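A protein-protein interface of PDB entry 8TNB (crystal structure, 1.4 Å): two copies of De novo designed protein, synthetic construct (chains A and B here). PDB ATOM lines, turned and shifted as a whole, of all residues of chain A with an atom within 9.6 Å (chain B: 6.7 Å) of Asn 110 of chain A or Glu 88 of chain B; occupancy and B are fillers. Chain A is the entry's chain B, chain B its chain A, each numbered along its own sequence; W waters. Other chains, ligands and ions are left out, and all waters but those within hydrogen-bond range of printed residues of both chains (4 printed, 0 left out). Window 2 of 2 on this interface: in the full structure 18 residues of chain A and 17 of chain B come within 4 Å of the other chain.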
ATOM      1  N   GLU A  40     -11.461   7.772  -3.583  1.00  0.00           N
ATOM      2  CA  GLU A  40     -12.162   8.983  -3.141  1.00  0.00           C
ATOM      3  C   GLU A  40     -11.229  10.164  -2.943  1.00  0.00           C
ATOM      4  O   GLU A  40     -11.632  11.312  -3.195  1.00  0.00           O
ATOM      5  CB  GLU A  40     -12.891   8.729  -1.818  1.00  0.00           C
ATOM      6  CG  GLU A  40     -14.046   7.802  -1.894  1.00  0.00           C
ATOM      7  CD  GLU A  40     -14.895   7.860  -0.622  1.00  0.00           C
ATOM      8  OE1 GLU A  40     -14.414   8.418   0.397  1.00  0.00           O
ATOM      9  OE2 GLU A  40     -16.017   7.361  -0.608  1.00  0.00           O
ATOM     10  N   ALA A  44     -11.512  13.667  -4.913  1.00  0.00           N
ATOM     11  CA  ALA A  44     -11.567  14.992  -4.296  1.00  0.00           C
ATOM     12  C   ALA A  44     -10.591  15.953  -4.950  1.00  0.00           C
ATOM     13  O   ALA A  44     -10.934  17.112  -5.210  1.00  0.00           O
ATOM     14  CB  ALA A  44     -11.258  14.880  -2.828  1.00  0.00           C
ATOM     15  N   LEU A  47     -11.866  16.879  -8.480  1.00  0.00           N
ATOM     16  CA  LEU A  47     -13.034  17.754  -8.403  1.00  0.00           C
ATOM     17  C   LEU A  47     -12.637  19.164  -8.004  1.00  0.00           C
ATOM     18  O   LEU A  47     -13.193  20.134  -8.539  1.00  0.00           O
ATOM     19  CB  LEU A  47     -14.024  17.162  -7.433  1.00  0.00           C
ATOM     20  CG  LEU A  47     -14.752  15.940  -8.005  1.00  0.00           C
ATOM     21  CD1 LEU A  47     -15.548  15.428  -6.845  1.00  0.00           C
ATOM     22  CD2 LEU A  47     -15.629  16.228  -9.209  1.00  0.00           C
ATOM     23  N   ASP A 102     -20.985  22.428  -8.716  1.00  0.00           N
ATOM     24  CA  ASP A 102     -21.062  22.659  -7.282  1.00  0.00           C
ATOM     25  C   ASP A 102     -21.866  21.560  -6.585  1.00  0.00           C
ATOM     26  O   ASP A 102     -21.471  21.052  -5.527  1.00  0.00           O
ATOM     27  CB  ASP A 102     -21.729  24.006  -6.969  1.00  0.00           C
ATOM     28  CG  ASP A 102     -20.806  25.200  -7.107  1.00  0.00           C
ATOM     29  OD1 ASP A 102     -19.577  25.021  -7.240  1.00  0.00           O
ATOM     30  OD2 ASP A 102     -21.363  26.338  -7.085  1.00  0.00           O
ATOM     31  N   THR A 103     -23.014  21.206  -7.167  1.00  0.00           N
ATOM     32  CA  THR A 103     -23.836  20.165  -6.569  1.00  0.00           C
ATOM     33  C   THR A 103     -23.077  18.856  -6.515  1.00  0.00           C
ATOM     34  O   THR A 103     -23.119  18.146  -5.510  1.00  0.00           O
ATOM     35  CB  THR A 103     -25.107  19.993  -7.390  1.00  0.00           C
ATOM     36  OG1 THR A 103     -25.829  21.224  -7.334  1.00  0.00           O
ATOM     37  CG2 THR A 103     -25.962  18.870  -6.835  1.00  0.00           C
ATOM     38  N   ALA A 104     -22.333  18.559  -7.577  1.00  0.00           N
ATOM     39  CA  ALA A 104     -21.566  17.314  -7.599  1.00  0.00           C
ATOM     40  C   ALA A 104     -20.431  17.312  -6.580  1.00  0.00           C
ATOM     41  O   ALA A 104     -20.211  16.317  -5.868  1.00  0.00           O
ATOM     42  CB  ALA A 104     -21.031  17.076  -8.997  1.00  0.00           C
ATOM     43  N   VAL A 105     -19.706  18.435  -6.469  1.00  0.00           N
ATOM     44  CA  VAL A 105     -18.626  18.522  -5.508  1.00  0.00           C
ATOM     45  C   VAL A 105     -19.151  18.361  -4.091  1.00  0.00           C
ATOM     46  O   VAL A 105     -18.542  17.664  -3.277  1.00  0.00           O
ATOM     47  CB  VAL A 105     -17.858  19.842  -5.709  1.00  0.00           C
ATOM     48  CG1 VAL A 105     -16.800  20.052  -4.652  1.00  0.00           C
ATOM     49  CG2 VAL A 105     -17.236  19.884  -7.083  1.00  0.00           C
ATOM     50  N   ALA A 106     -20.265  19.021  -3.764  1.00  0.00           N
ATOM     51  CA  ALA A 106     -20.803  18.880  -2.423  1.00  0.00           C
ATOM     52  C   ALA A 106     -21.266  17.464  -2.159  1.00  0.00           C
ATOM     53  O   ALA A 106     -21.089  16.947  -1.057  1.00  0.00           O
ATOM     54  CB  ALA A 106     -21.966  19.847  -2.222  1.00  0.00           C
ATOM     55  N   ALA A 107     -21.901  16.841  -3.145  1.00  0.00           N
ATOM     56  CA  ALA A 107     -22.376  15.478  -2.945  1.00  0.00           C
ATOM     57  C   ALA A 107     -21.213  14.535  -2.696  1.00  0.00           C
ATOM     58  O   ALA A 107     -21.294  13.651  -1.827  1.00  0.00           O
ATOM     59  CB  ALA A 107     -23.177  15.026  -4.154  1.00  0.00           C
ATOM     60  N   ALA A 108     -20.117  14.691  -3.452  1.00  0.00           N
ATOM     61  CA  ALA A 108     -18.946  13.852  -3.205  1.00  0.00           C
ATOM     62  C   ALA A 108     -18.380  14.089  -1.811  1.00  0.00           C
ATOM     63  O   ALA A 108     -17.903  13.158  -1.159  1.00  0.00           O
ATOM     64  CB  ALA A 108     -17.857  14.108  -4.244  1.00  0.00           C
ATOM     65  N   ALA A 109     -18.374  15.343  -1.343  1.00  0.00           N
ATOM     66  CA  ALA A 109     -17.841  15.599  -0.013  1.00  0.00           C
ATOM     67  C   ALA A 109     -18.755  15.025   1.070  1.00  0.00           C
ATOM     68  O   ALA A 109     -18.275  14.605   2.126  1.00  0.00           O
ATOM     69  CB  ALA A 109     -17.674  17.116   0.197  1.00  0.00           C
ATOM     70  N   ASN A 110     -20.071  15.068   0.833  1.00  0.00           N
ATOM     71  CA  ASN A 110     -21.099  14.572   1.743  1.00  0.00           C
ATOM     72  C   ASN A 110     -21.247  13.063   1.684  1.00  0.00           C
ATOM     73  O   ASN A 110     -22.024  12.502   2.464  1.00  0.00           O
ATOM     74  CB  ASN A 110     -22.490  15.132   1.341  1.00  0.00           C
ATOM     75  CG  ASN A 110     -22.828  16.472   1.993  1.00  0.00           C
ATOM     76  OD1 ASN A 110     -23.686  16.561   2.890  1.00  0.00           O
ATOM     77  ND2 ASN A 110     -22.225  17.534   1.480  1.00  0.00           N
ATOM     78  N   GLY A 111     -20.547  12.405   0.771  1.00  0.00           N
ATOM     79  CA  GLY A 111     -20.723  10.975   0.566  1.00  0.00           C
ATOM     80  C   GLY A 111     -22.120  10.605   0.106  1.00  0.00           C
ATOM     81  O   GLY A 111     -22.771   9.725   0.689  1.00  0.00           O
ATOM     82  N   ASP A 112     -22.597  11.270  -0.951  1.00  0.00           N
ATOM     83  CA  ASP A 112     -23.927  11.055  -1.526  1.00  0.00           C
ATOM     84  C   ASP A 112     -23.721  10.799  -3.023  1.00  0.00           C
ATOM     85  O   ASP A 112     -23.871  11.701  -3.851  1.00  0.00           O
ATOM     86  CB  ASP A 112     -24.833  12.291  -1.253  1.00  0.00           C
ATOM     87  CG  ASP A 112     -26.205  12.178  -1.899  1.00  0.00           C
ATOM     88  OD1 ASP A 112     -26.504  11.132  -2.506  1.00  0.00           O
ATOM     89  OD2 ASP A 112     -26.993  13.151  -1.813  1.00  0.00           O
ATOM     90  N   GLU A 113     -23.372   9.552  -3.380  1.00  0.00           N
ATOM     91  CA  GLU A 113     -23.042   9.271  -4.772  1.00  0.00           C
ATOM     92  C   GLU A 113     -24.245   9.374  -5.695  1.00  0.00           C
ATOM     93  O   GLU A 113     -24.097   9.799  -6.841  1.00  0.00           O
ATOM     94  CB  GLU A 113     -22.328   7.929  -4.928  1.00  0.00           C
ATOM     95  CG  GLU A 113     -21.397   7.631  -3.785  1.00  0.00           C
ATOM     96  CD  GLU A 113     -20.449   6.490  -4.104  1.00  0.00           C
ATOM     97  OE1 GLU A 113     -20.886   5.526  -4.781  1.00  0.00           O
ATOM     98  OE2 GLU A 113     -19.274   6.570  -3.681  1.00  0.00           O
ATOM     99  N   GLU A 114     -25.437   9.025  -5.241  1.00  0.00           N
ATOM    100  CA  GLU A 114     -26.588   9.153  -6.125  1.00  0.00           C
ATOM    101  C   GLU A 114     -26.695  10.585  -6.648  1.00  0.00           C
ATOM    102  O   GLU A 114     -26.834  10.806  -7.855  1.00  0.00           O
ATOM    103  CB  GLU A 114     -27.848   8.703  -5.390  1.00  0.00           C
ATOM    104  CG  GLU A 114     -29.148   9.074  -6.075  1.00  0.00           C
ATOM    105  CD  GLU A 114     -30.350   8.382  -5.445  1.00  0.00           C
ATOM    106  OE1 GLU A 114     -30.399   8.280  -4.198  1.00  0.00           O
ATOM    107  OE2 GLU A 114     -31.243   7.942  -6.201  1.00  0.00           O
ATOM    108  N   THR A 115     -26.574  11.572  -5.759  1.00  0.00           N
ATOM    109  CA  THR A 115     -26.597  12.958  -6.208  1.00  0.00           C
ATOM    110  C   THR A 115     -25.360  13.290  -7.029  1.00  0.00           C
ATOM    111  O   THR A 115     -25.463  13.992  -8.042  1.00  0.00           O
ATOM    112  CB  THR A 115     -26.722  13.870  -4.994  1.00  0.00           C
ATOM    113  OG1 THR A 115     -27.946  13.558  -4.310  1.00  0.00           O
ATOM    114  CG2 THR A 115     -26.718  15.330  -5.401  1.00  0.00           C
ATOM    115  N   PHE A 116     -24.193  12.789  -6.610  1.00  0.00           N
ATOM    116  CA  PHE A 116     -22.955  13.101  -7.325  1.00  0.00           C
ATOM    117  C   PHE A 116     -23.026  12.650  -8.776  1.00  0.00           C
ATOM    118  O   PHE A 116     -22.730  13.409  -9.699  1.00  0.00           O
ATOM    119  CB  PHE A 116     -21.732  12.463  -6.660  1.00  0.00           C
ATOM    120  CG  PHE A 116     -20.518  12.498  -7.535  1.00  0.00           C
ATOM    121  CD1 PHE A 116     -19.773  13.675  -7.676  1.00  0.00           C
ATOM    122  CD2 PHE A 116     -20.153  11.391  -8.296  1.00  0.00           C
ATOM    123  CE1 PHE A 116     -18.695  13.726  -8.513  1.00  0.00           C
ATOM    124  CE2 PHE A 116     -19.067  11.445  -9.116  1.00  0.00           C
ATOM    125  CZ  PHE A 116     -18.340  12.594  -9.249  1.00  0.00           C
ATOM    126  N   ALA B  61     -15.186  25.560   2.259  1.00  0.00           N
ATOM    127  CA  ALA B  61     -16.377  24.930   2.811  1.00  0.00           C
ATOM    128  C   ALA B  61     -16.445  23.454   2.416  1.00  0.00           C
ATOM    129  O   ALA B  61     -16.777  22.595   3.251  1.00  0.00           O
ATOM    130  CB  ALA B  61     -17.622  25.686   2.385  1.00  0.00           C
ATOM    131  N   VAL B  65     -16.143  20.186   5.123  1.00  0.00           N
ATOM    132  CA  VAL B  65     -16.985  18.996   5.113  1.00  0.00           C
ATOM    133  C   VAL B  65     -16.116  17.741   5.009  1.00  0.00           C
ATOM    134  O   VAL B  65     -16.299  16.775   5.766  1.00  0.00           O
ATOM    135  CB  VAL B  65     -18.045  19.079   4.004  1.00  0.00           C
ATOM    136  CG1 VAL B  65     -18.731  17.734   3.802  1.00  0.00           C
ATOM    137  CG2 VAL B  65     -19.092  20.144   4.348  1.00  0.00           C
ATOM    138  N   ARG B  66     -15.138  17.744   4.099  1.00  0.00           N
ATOM    139  CA  ARG B  66     -14.316  16.539   3.934  1.00  0.00           C
ATOM    140  C   ARG B  66     -13.544  16.202   5.205  1.00  0.00           C
ATOM    141  O   ARG B  66     -13.459  15.023   5.593  1.00  0.00           O
ATOM    142  CB  ARG B  66     -13.353  16.688   2.767  1.00  0.00           C
ATOM    143  CG  ARG B  66     -14.012  16.609   1.420  1.00  0.00           C
ATOM    144  CD  ARG B  66     -12.941  16.909   0.405  1.00  0.00           C
ATOM    145  NE  ARG B  66     -13.439  17.221  -0.921  1.00  0.00           N
ATOM    146  CZ  ARG B  66     -12.769  17.973  -1.785  1.00  0.00           C
ATOM    147  NH1 ARG B  66     -11.626  18.550  -1.447  1.00  0.00           N
ATOM    148  NH2 ARG B  66     -13.276  18.172  -3.001  1.00  0.00           N
ATOM    149  N   LEU B  68     -14.358  17.017   8.348  1.00  0.00           N
ATOM    150  CA  LEU B  68     -15.262  16.559   9.394  1.00  0.00           C
ATOM    151  C   LEU B  68     -15.762  15.157   9.110  1.00  0.00           C
ATOM    152  O   LEU B  68     -15.888  14.356  10.046  1.00  0.00           O
ATOM    153  CB  LEU B  68     -16.412  17.553   9.583  1.00  0.00           C
ATOM    154  CG  LEU B  68     -15.921  18.733  10.392  1.00  0.00           C
ATOM    155  CD1 LEU B  68     -16.872  19.880  10.193  1.00  0.00           C
ATOM    156  CD2 LEU B  68     -15.840  18.372  11.877  1.00  0.00           C
ATOM    157  N   ALA B  69     -16.041  14.838   7.829  1.00  0.00           N
ATOM    158  CA  ALA B  69     -16.317  13.453   7.432  1.00  0.00           C
ATOM    159  C   ALA B  69     -15.205  12.514   7.881  1.00  0.00           C
ATOM    160  O   ALA B  69     -15.472  11.432   8.423  1.00  0.00           O
ATOM    161  CB  ALA B  69     -16.492  13.370   5.915  1.00  0.00           C
ATOM    162  N   ASP B  81     -20.883  14.004  14.626  1.00  0.00           N
ATOM    163  CA  ASP B  81     -22.068  14.028  13.787  1.00  0.00           C
ATOM    164  C   ASP B  81     -22.624  15.436  13.656  1.00  0.00           C
ATOM    165  O   ASP B  81     -22.945  15.885  12.550  1.00  0.00           O
ATOM    166  CB  ASP B  81     -23.122  13.092  14.393  1.00  0.00           C
ATOM    167  CG  ASP B  81     -23.919  12.340  13.347  1.00  0.00           C
ATOM    168  OD1 ASP B  81     -24.486  12.990  12.443  1.00  0.00           O
ATOM    169  OD2 ASP B  81     -23.983  11.093  13.427  1.00  0.00           O
ATOM    170  N   ALA B  83     -21.212  18.456  14.271  1.00  0.00           N
ATOM    171  CA  ALA B  83     -20.306  19.349  13.552  1.00  0.00           C
ATOM    172  C   ALA B  83     -20.412  19.117  12.052  1.00  0.00           C
ATOM    173  O   ALA B  83     -20.532  20.068  11.277  1.00  0.00           O
ATOM    174  CB  ALA B  83     -18.871  19.164  14.010  1.00  0.00           C
ATOM    175  N   LEU B  84     -20.351  17.854  11.622  1.00  0.00           N
ATOM    176  CA  LEU B  84     -20.509  17.564  10.193  1.00  0.00           C
ATOM    177  C   LEU B  84     -21.832  18.087   9.639  1.00  0.00           C
ATOM    178  O   LEU B  84     -21.870  18.657   8.538  1.00  0.00           O
ATOM    179  CB  LEU B  84     -20.371  16.059   9.930  1.00  0.00           C
ATOM    180  CG  LEU B  84     -20.589  15.652   8.488  1.00  0.00           C
ATOM    181  CD1 LEU B  84     -19.455  16.183   7.630  1.00  0.00           C
ATOM    182  CD2 LEU B  84     -20.685  14.116   8.383  1.00  0.00           C
ATOM    183  N   GLN B  85     -22.931  17.907  10.378  1.00  0.00           N
ATOM    184  CA  GLN B  85     -24.229  18.379   9.889  1.00  0.00           C
ATOM    185  C   GLN B  85     -24.215  19.903   9.715  1.00  0.00           C
ATOM    186  O   GLN B  85     -24.759  20.415   8.725  1.00  0.00           O
ATOM    187  CB  GLN B  85     -25.359  17.973  10.837  1.00  0.00           C
ATOM    188  CG  GLN B  85     -25.546  16.466  11.058  1.00  0.00           C
ATOM    189  CD  GLN B  85     -25.368  15.630   9.799  1.00  0.00           C
ATOM    190  OE1 GLN B  85     -26.038  15.854   8.783  1.00  0.00           O
ATOM    191  NE2 GLN B  85     -24.469  14.658   9.859  1.00  0.00           N
ATOM    192  N   ILE B  86     -23.632  20.623  10.664  1.00  0.00           N
ATOM    193  CA  ILE B  86     -23.525  22.076  10.525  1.00  0.00           C
ATOM    194  C   ILE B  86     -22.697  22.415   9.292  1.00  0.00           C
ATOM    195  O   ILE B  86     -23.055  23.299   8.493  1.00  0.00           O
ATOM    196  CB  ILE B  86     -22.892  22.675  11.785  1.00  0.00           C
ATOM    197  CG1 ILE B  86     -23.796  22.492  13.006  1.00  0.00           C
ATOM    198  CG2 ILE B  86     -22.615  24.157  11.609  1.00  0.00           C
ATOM    199  CD1 ILE B  86     -23.032  22.702  14.310  1.00  0.00           C
ATOM    200  N   ALA B  87     -21.556  21.744   9.146  1.00  0.00           N
ATOM    201  CA  ALA B  87     -20.666  22.054   8.029  1.00  0.00           C
ATOM    202  C   ALA B  87     -21.324  21.759   6.699  1.00  0.00           C
ATOM    203  O   ALA B  87     -21.110  22.477   5.732  1.00  0.00           O
ATOM    204  CB  ALA B  87     -19.372  21.248   8.159  1.00  0.00           C
ATOM    205  N   GLU B  88     -22.148  20.707   6.621  1.00  0.00           N
ATOM    206  CA  GLU B  88     -22.861  20.431   5.379  1.00  0.00           C
ATOM    207  C   GLU B  88     -23.918  21.502   5.093  1.00  0.00           C
ATOM    208  O   GLU B  88     -24.137  21.879   3.933  1.00  0.00           O
ATOM    209  CB  GLU B  88     -23.465  19.019   5.464  1.00  0.00           C
ATOM    210  CG  GLU B  88     -22.373  17.965   5.446  1.00  0.00           C
ATOM    211  CD  GLU B  88     -22.866  16.555   5.642  1.00  0.00           C
ATOM    212  OE1 GLU B  88     -24.025  16.387   6.072  1.00  0.00           O
ATOM    213  OE2 GLU B  88     -22.072  15.621   5.351  1.00  0.00           O
ATOM    214  N   LYS B  89     -24.595  22.009   6.128  1.00  0.00           N
ATOM    215  CA  LYS B  89     -25.534  23.105   5.902  1.00  0.00           C
ATOM    216  C   LYS B  89     -24.797  24.389   5.520  1.00  0.00           C
ATOM    217  O   LYS B  89     -25.251  25.133   4.639  1.00  0.00           O
ATOM    218  CB  LYS B  89     -26.384  23.308   7.165  1.00  0.00           C
ATOM    219  CG  LYS B  89     -27.355  24.483   7.118  1.00  0.00           C
ATOM    220  CD  LYS B  89     -28.631  24.208   6.326  1.00  0.00           C
ATOM    221  CE  LYS B  89     -29.822  25.087   6.790  1.00  0.00           C
ATOM    222  NZ  LYS B  89     -29.782  25.536   8.220  1.00  0.00           N
ATOM    223  N   LEU B  90     -23.642  24.636   6.148  1.00  0.00           N
ATOM    224  CA  LEU B  90     -22.797  25.759   5.730  1.00  0.00           C
ATOM    225  C   LEU B  90     -22.435  25.654   4.258  1.00  0.00           C
ATOM    226  O   LEU B  90     -22.553  26.622   3.507  1.00  0.00           O
ATOM    227  CB  LEU B  90     -21.557  25.812   6.600  1.00  0.00           C
ATOM    228  CG  LEU B  90     -20.501  26.843   6.213  1.00  0.00           C
ATOM    229  CD1 LEU B  90     -21.003  28.302   6.201  1.00  0.00           C
ATOM    230  CD2 LEU B  90     -19.286  26.695   7.132  1.00  0.00           C
ATOM    231  N   LEU B  91     -21.981  24.470   3.822  1.00  0.00           N
ATOM    232  CA  LEU B  91     -21.599  24.317   2.430  1.00  0.00           C
ATOM    233  C   LEU B  91     -22.784  24.565   1.512  1.00  0.00           C
ATOM    234  O   LEU B  91     -22.655  25.231   0.485  1.00  0.00           O
ATOM    235  CB  LEU B  91     -21.013  22.915   2.243  1.00  0.00           C
ATOM    236  CG  LEU B  91     -20.653  22.575   0.804  1.00  0.00           C
ATOM    237  CD1 LEU B  91     -19.669  23.536   0.182  1.00  0.00           C
ATOM    238  CD2 LEU B  91     -20.148  21.136   0.726  1.00  0.00           C
ATOM    239  N   LYS B  92     -23.967  24.051   1.866  1.00  0.00           N
ATOM    240  CA  LYS B  92     -25.145  24.251   1.032  1.00  0.00           C
ATOM    241  C   LYS B  92     -25.460  25.730   0.883  1.00  0.00           C
ATOM    242  O   LYS B  92     -25.743  26.214  -0.219  1.00  0.00           O
ATOM    243  CB  LYS B  92     -26.314  23.527   1.692  1.00  0.00           C
ATOM    244  CG  LYS B  92     -27.617  23.699   0.967  1.00  0.00           C
ATOM    245  CD  LYS B  92     -28.710  22.740   1.484  1.00  0.00           C
ATOM    246  CE  LYS B  92     -29.986  22.844   0.647  1.00  0.00           C
ATOM    247  NZ  LYS B  92     -30.948  21.716   0.882  1.00  0.00           N
ATOM    248  N   THR B  93     -25.332  26.458   1.993  1.00  0.00           N
ATOM    249  CA  THR B  93     -25.651  27.876   1.985  1.00  0.00           C
ATOM    250  C   THR B  93     -24.617  28.665   1.197  1.00  0.00           C
ATOM    251  O   THR B  93     -24.976  29.554   0.409  1.00  0.00           O
ATOM    252  CB  THR B  93     -25.703  28.360   3.419  1.00  0.00           C
ATOM    253  OG1 THR B  93     -26.639  27.559   4.160  1.00  0.00           O
ATOM    254  CG2 THR B  93     -26.144  29.805   3.508  1.00  0.00           C
HETATM  255  O   HOH W   1     -14.889  14.622  -1.801  1.00  0.00           O
HETATM  256  O   HOH W   2     -26.053  17.111   3.429  1.00  0.00           O
HETATM  257  O   HOH W   3     -15.758  16.885  -3.221  1.00  0.00           O
HETATM  258  O   HOH W   4     -23.636  20.392   1.673  1.00  0.00           O
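No position is printed for both chains. Of the 5 pairs that touch across the chains among the printed residues, none has its exchanged pair printed and touching as well.
Of the printed residues of chain B, Ala 106 of chain A touches Leu 91. Of the printed residues of chain B, Asn 110 of chain A touches Glu 88. Of the printed residues of chain A, Val 65 of chain B touches Ala 109. Of the printed residues of chain A, Arg 66 of chain B touches Ala 44 and Ala 109. No residue of chain A comes within 4 Å of Gln 85 of chain B. No residue of chain A comes within 4 Å of Ala 87 of chain B. Of chain A, only Asn 110 comes within 4 Å of Glu 88 of chain B. The nearest residue of chain A that does not touch Glu 88 of chain B is Ala 109 of chain A (5.1 Å). The nearest printed residue of chain A that does not touch Val 65 of chain B is Asn 110 of chain A (4.2 Å).
Leu 91 of chain B touches Ala 106 of chain A (CD2 to CB, 3.7 Å). Val 65 of chain B touches Ala 109 of chain A (CG1 to O, 3.6 Å). CB of Ala 109 of chain A touches CG of Arg 66 of chain B (3.9 Å).
Water W2 lies within hydrogen-bond range of OD1 of Asn 110 of chain A (2.5 Å) and OE1 of Glu 88 of chain B (3.4 Å). Water W4 bridges the backbone carbonyl oxygen (O) of Glu 88 of chain B (2.8 Å) and the side-chain amide nitrogen (ND2) of Asn 110 of chain A (3.2 Å). Water W3 lies within hydrogen-bond range of NH2 of Arg 66 of chain B and O of Val 105 of chain A. Water W1 bridges the guanidinium group (NE) of Arg 66 of chain B (3.1 Å) and the backbone carbonyl oxygen (O) of Ala 108 of chain A (3.4 Å).
The side-chain amide oxygen (OE1) of Gln 85 of chain B lies close to the side-chain carboxylate (OE1) of Glu 88 of chain B, 3.4 Å away. The side-chain amide nitrogen (ND2) of Asn 110 of chain A lies within hydrogen-bond range of the backbone carbonyl oxygen (O) of Ala 106 of chain A (2.8 Å).
NH2 of Arg 66 of chain B sits at hydrogen-bond distance from O of Ala 44 of chain A (3.4 Å). OE2 of Glu 88 of chain B lies close to OD1 of Asn 110 of chain A, at 3.1 Å.
Hydrophobic or aromatic side chains of chain A within 4 Å of the printed part of chain B: Ala 44, Ala 106 and Ala 109. Among the printed residues, 5 pairs touch across the chains. Among the printed residues, no Asp or Glu carboxylate lies within 4 Å of a Lys or Arg side-chain nitrogen of the other chain.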
